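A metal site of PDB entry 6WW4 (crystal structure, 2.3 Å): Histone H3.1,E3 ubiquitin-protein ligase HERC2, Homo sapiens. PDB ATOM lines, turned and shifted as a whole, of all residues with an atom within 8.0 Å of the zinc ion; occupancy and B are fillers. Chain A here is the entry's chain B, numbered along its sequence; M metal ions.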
ATOM      1  N   LYS A  27     -17.546  -4.245  20.731  1.00  0.00           N
ATOM      2  CA  LYS A  27     -17.471  -3.479  19.492  1.00  0.00           C
ATOM      3  C   LYS A  27     -16.898  -2.105  19.769  1.00  0.00           C
ATOM      4  O   LYS A  27     -17.334  -1.422  20.700  1.00  0.00           O
ATOM      5  CB  LYS A  27     -18.855  -3.341  18.848  1.00  0.00           C
ATOM      6  CG  LYS A  27     -18.867  -2.461  17.609  1.00  0.00           C
ATOM      7  CD  LYS A  27     -20.240  -2.516  16.917  1.00  0.00           C
ATOM      8  CE  LYS A  27     -20.323  -1.647  15.641  1.00  0.00           C
ATOM      9  NZ  LYS A  27     -19.308  -1.978  14.578  1.00  0.00           N
ATOM     10  N   CYS A  28     -15.934  -1.695  18.968  1.00  0.00           N
ATOM     11  CA  CYS A  28     -15.443  -0.326  19.134  1.00  0.00           C
ATOM     12  C   CYS A  28     -16.543   0.658  18.785  1.00  0.00           C
ATOM     13  O   CYS A  28     -17.249   0.504  17.785  1.00  0.00           O
ATOM     14  CB  CYS A  28     -14.216  -0.062  18.274  1.00  0.00           C
ATOM     15  SG  CYS A  28     -13.543   1.583  18.561  1.00  0.00           S
ATOM     16  N   ARG A  29     -16.704   1.668  19.637  1.00  0.00           N
ATOM     17  CA  ARG A  29     -17.688   2.713  19.434  1.00  0.00           C
ATOM     18  C   ARG A  29     -17.173   3.839  18.537  1.00  0.00           C
ATOM     19  O   ARG A  29     -17.957   4.683  18.117  1.00  0.00           O
ATOM     20  CB  ARG A  29     -18.153   3.266  20.777  1.00  0.00           C
ATOM     21  CG  ARG A  29     -18.620   2.175  21.773  1.00  0.00           C
ATOM     22  CD  ARG A  29     -18.866   2.728  23.171  1.00  0.00           C
ATOM     23  NE  ARG A  29     -20.024   3.631  23.229  1.00  0.00           N
ATOM     24  CZ  ARG A  29     -19.982   4.880  23.675  1.00  0.00           C
ATOM     25  NH1 ARG A  29     -21.086   5.608  23.691  1.00  0.00           N
ATOM     26  NH2 ARG A  29     -18.844   5.382  24.141  1.00  0.00           N
ATOM     27  N   ASN A  30     -15.881   3.831  18.208  1.00  0.00           N
ATOM     28  CA  ASN A  30     -15.257   4.825  17.339  1.00  0.00           C
ATOM     29  C   ASN A  30     -14.866   4.277  15.972  1.00  0.00           C
ATOM     30  O   ASN A  30     -15.089   4.951  14.968  1.00  0.00           O
ATOM     31  CB  ASN A  30     -14.009   5.420  18.008  1.00  0.00           C
ATOM     32  CG  ASN A  30     -14.308   6.029  19.355  1.00  0.00           C
ATOM     33  OD1 ASN A  30     -14.314   5.338  20.372  1.00  0.00           O
ATOM     34  ND2 ASN A  30     -14.561   7.325  19.378  1.00  0.00           N
ATOM     35  N   CYS A  31     -14.279   3.089  15.897  1.00  0.00           N
ATOM     36  CA  CYS A  31     -14.045   2.463  14.604  1.00  0.00           C
ATOM     37  C   CYS A  31     -15.358   2.077  13.966  1.00  0.00           C
ATOM     38  O   CYS A  31     -16.353   1.790  14.656  1.00  0.00           O
ATOM     39  CB  CYS A  31     -13.163   1.223  14.748  1.00  0.00           C
ATOM     40  SG  CYS A  31     -11.457   1.539  15.216  1.00  0.00           S
ATOM     41  N   ASP A  32     -15.370   2.026  12.640  1.00  0.00           N
ATOM     42  CA  ASP A  32     -16.602   1.644  11.968  1.00  0.00           C
ATOM     43  C   ASP A  32     -16.982   0.196  12.235  1.00  0.00           C
ATOM     44  O   ASP A  32     -18.158  -0.096  12.450  1.00  0.00           O
ATOM     45  CB  ASP A  32     -16.498   1.863  10.466  1.00  0.00           C
ATOM     46  CG  ASP A  32     -17.780   1.499   9.760  1.00  0.00           C
ATOM     47  OD1 ASP A  32     -18.801   2.189   9.973  1.00  0.00           O
ATOM     48  OD2 ASP A  32     -17.778   0.534   8.990  1.00  0.00           O
ATOM     49  N   ASP A  33     -16.009  -0.714  12.219  1.00  0.00           N
ATOM     50  CA  ASP A  33     -16.284  -2.157  12.118  1.00  0.00           C
ATOM     51  C   ASP A  33     -15.138  -2.931  12.783  1.00  0.00           C
ATOM     52  O   ASP A  33     -14.455  -3.739  12.148  1.00  0.00           O
ATOM     53  CB  ASP A  33     -16.480  -2.537  10.654  1.00  0.00           C
ATOM     54  CG  ASP A  33     -16.856  -4.022  10.435  1.00  0.00           C
ATOM     55  OD1 ASP A  33     -16.338  -4.619   9.466  1.00  0.00           O
ATOM     56  OD2 ASP A  33     -17.679  -4.590  11.193  1.00  0.00           O
ATOM     57  N   PHE A  34     -14.913  -2.693  14.075  1.00  0.00           N
ATOM     58  CA  PHE A  34     -13.811  -3.316  14.831  1.00  0.00           C
ATOM     59  C   PHE A  34     -14.378  -3.982  16.080  1.00  0.00           C
ATOM     60  O   PHE A  34     -15.121  -3.341  16.842  1.00  0.00           O
ATOM     61  CB  PHE A  34     -12.747  -2.264  15.210  1.00  0.00           C
ATOM     62  CG  PHE A  34     -11.534  -2.851  15.900  1.00  0.00           C
ATOM     63  CD1 PHE A  34     -11.593  -3.275  17.218  1.00  0.00           C
ATOM     64  CD2 PHE A  34     -10.317  -2.974  15.227  1.00  0.00           C
ATOM     65  CE1 PHE A  34     -10.469  -3.810  17.855  1.00  0.00           C
ATOM     66  CE2 PHE A  34      -9.197  -3.512  15.850  1.00  0.00           C
ATOM     67  CZ  PHE A  34      -9.270  -3.936  17.164  1.00  0.00           C
ATOM     68  N   ASP A  35     -14.033  -5.249  16.303  1.00  0.00           N
ATOM     69  CA  ASP A  35     -14.575  -6.035  17.400  1.00  0.00           C
ATOM     70  C   ASP A  35     -13.487  -6.840  18.089  1.00  0.00           C
ATOM     71  O   ASP A  35     -12.530  -7.292  17.468  1.00  0.00           O
ATOM     72  CB  ASP A  35     -15.682  -6.994  16.928  1.00  0.00           C
ATOM     73  CG  ASP A  35     -16.898  -6.278  16.366  1.00  0.00           C
ATOM     74  OD1 ASP A  35     -16.976  -6.116  15.131  1.00  0.00           O
ATOM     75  OD2 ASP A  35     -17.769  -5.880  17.172  1.00  0.00           O
ATOM     76  N   HIS A  46      -5.822  -1.071  21.965  1.00  0.00           N
ATOM     77  CA  HIS A  46      -6.442  -0.584  20.740  1.00  0.00           C
ATOM     78  C   HIS A  46      -6.080   0.889  20.632  1.00  0.00           C
ATOM     79  O   HIS A  46      -4.911   1.250  20.797  1.00  0.00           O
ATOM     80  CB  HIS A  46      -7.950  -0.843  20.767  1.00  0.00           C
ATOM     81  CG  HIS A  46      -8.675  -0.451  19.520  1.00  0.00           C
ATOM     82  ND1 HIS A  46      -8.327  -0.919  18.268  1.00  0.00           N
ATOM     83  CD2 HIS A  46      -9.727   0.375  19.331  1.00  0.00           C
ATOM     84  CE1 HIS A  46      -9.130  -0.395  17.370  1.00  0.00           C
ATOM     85  NE2 HIS A  46      -9.988   0.399  17.978  1.00  0.00           N
ATOM     86  N   ASN A  47      -7.030   1.770  20.383  1.00  0.00           N
ATOM     87  CA  ASN A  47      -6.724   3.183  20.352  1.00  0.00           C
ATOM     88  C   ASN A  47      -7.130   3.762  21.693  1.00  0.00           C
ATOM     89  O   ASN A  47      -8.288   3.632  22.099  1.00  0.00           O
ATOM     90  CB  ASN A  47      -7.447   3.884  19.190  1.00  0.00           C
ATOM     91  CG  ASN A  47      -7.023   5.322  19.011  1.00  0.00           C
ATOM     92  OD1 ASN A  47      -7.053   6.119  19.951  1.00  0.00           O
ATOM     93  ND2 ASN A  47      -6.659   5.684  17.782  1.00  0.00           N
ATOM     94  N   THR A  48      -6.178   4.391  22.375  1.00  0.00           N
ATOM     95  CA  THR A  48      -6.414   4.832  23.736  1.00  0.00           C
ATOM     96  C   THR A  48      -7.596   5.782  23.829  1.00  0.00           C
ATOM     97  O   THR A  48      -8.253   5.860  24.859  1.00  0.00           O
ATOM     98  CB  THR A  48      -5.131   5.451  24.320  1.00  0.00           C
ATOM     99  OG1 THR A  48      -5.408   6.020  25.610  1.00  0.00           O
ATOM    100  CG2 THR A  48      -4.606   6.549  23.411  1.00  0.00           C
ATOM    101  N   ARG A  49      -7.890   6.509  22.757  1.00  0.00           N
ATOM    102  CA  ARG A  49      -9.064   7.374  22.732  1.00  0.00           C
ATOM    103  C   ARG A  49     -10.337   6.649  22.315  1.00  0.00           C
ATOM    104  O   ARG A  49     -11.402   7.270  22.231  1.00  0.00           O
ATOM    105  CB  ARG A  49      -8.815   8.571  21.792  1.00  0.00           C
ATOM    106  CG  ARG A  49      -7.790   9.576  22.301  1.00  0.00           C
ATOM    107  CD  ARG A  49      -8.430  10.916  22.560  1.00  0.00           C
ATOM    108  NE  ARG A  49      -9.183  11.387  21.401  1.00  0.00           N
ATOM    109  CZ  ARG A  49     -10.178  12.270  21.445  1.00  0.00           C
ATOM    110  NH1 ARG A  49     -10.801  12.622  20.322  1.00  0.00           N
ATOM    111  NH2 ARG A  49     -10.558  12.803  22.593  1.00  0.00           N
ATOM    112  N   HIS A  50     -10.263   5.348  22.044  1.00  0.00           N
ATOM    113  CA  HIS A  50     -11.429   4.610  21.605  1.00  0.00           C
ATOM    114  C   HIS A  50     -12.025   3.839  22.767  1.00  0.00           C
ATOM    115  O   HIS A  50     -11.324   3.438  23.697  1.00  0.00           O
ATOM    116  CB  HIS A  50     -11.066   3.673  20.438  1.00  0.00           C
ATOM    117  CG  HIS A  50     -10.876   4.389  19.146  1.00  0.00           C
ATOM    118  ND1 HIS A  50     -10.985   3.771  17.918  1.00  0.00           N
ATOM    119  CD2 HIS A  50     -10.597   5.688  18.879  1.00  0.00           C
ATOM    120  CE1 HIS A  50     -10.776   4.650  16.960  1.00  0.00           C
ATOM    121  NE2 HIS A  50     -10.534   5.825  17.515  1.00  0.00           N
ATOM    122  N   THR A  51     -13.343   3.654  22.734  1.00  0.00           N
ATOM    123  CA  THR A  51     -14.047   2.962  23.804  1.00  0.00           C
ATOM    124  C   THR A  51     -14.930   1.886  23.194  1.00  0.00           C
ATOM    125  O   THR A  51     -15.465   2.053  22.095  1.00  0.00           O
ATOM    126  CB  THR A  51     -14.886   3.938  24.659  1.00  0.00           C
ATOM    127  OG1 THR A  51     -13.999   4.803  25.402  1.00  0.00           O
ATOM    128  CG2 THR A  51     -15.772   3.200  25.644  1.00  0.00           C
ATOM    129  N   PHE A  52     -15.090   0.783  23.925  1.00  0.00           N
ATOM    130  CA  PHE A  52     -15.811  -0.386  23.454  1.00  0.00           C
ATOM    131  C   PHE A  52     -17.133  -0.508  24.196  1.00  0.00           C
ATOM    132  O   PHE A  52     -17.228  -0.248  25.398  1.00  0.00           O
ATOM    133  CB  PHE A  52     -14.989  -1.664  23.663  1.00  0.00           C
ATOM    134  CG  PHE A  52     -13.834  -1.808  22.710  1.00  0.00           C
ATOM    135  CD1 PHE A  52     -12.669  -1.071  22.892  1.00  0.00           C
ATOM    136  CD2 PHE A  52     -13.907  -2.688  21.655  1.00  0.00           C
ATOM    137  CE1 PHE A  52     -11.610  -1.210  22.005  1.00  0.00           C
ATOM    138  CE2 PHE A  52     -12.859  -2.840  20.781  1.00  0.00           C
ATOM    139  CZ  PHE A  52     -11.711  -2.089  20.942  1.00  0.00           C
HETATM  140 ZN    ZN M   1     -11.514   1.695  17.524  1.00  0.00          ZN
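The backbone NH (N) of Cys 28 sits at hydrogen-bond distance from the backbone carbonyl oxygen (O) of Phe 34 (2.8 Å).
N of Asn 30 sits close to SG of Cys 28 (3.3 Å).
Of the 16 residues printed, 4 come within 4 Å of the zinc ion.
The zinc ion is bound by NE2 of His 46 (2.1 Å), ND1 of His 50 (2.2 Å), SG of Cys 28 (2.3 Å) and SG of Cys 31 (2.3 Å).
The zinc ion has four donor atoms within binding distance.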
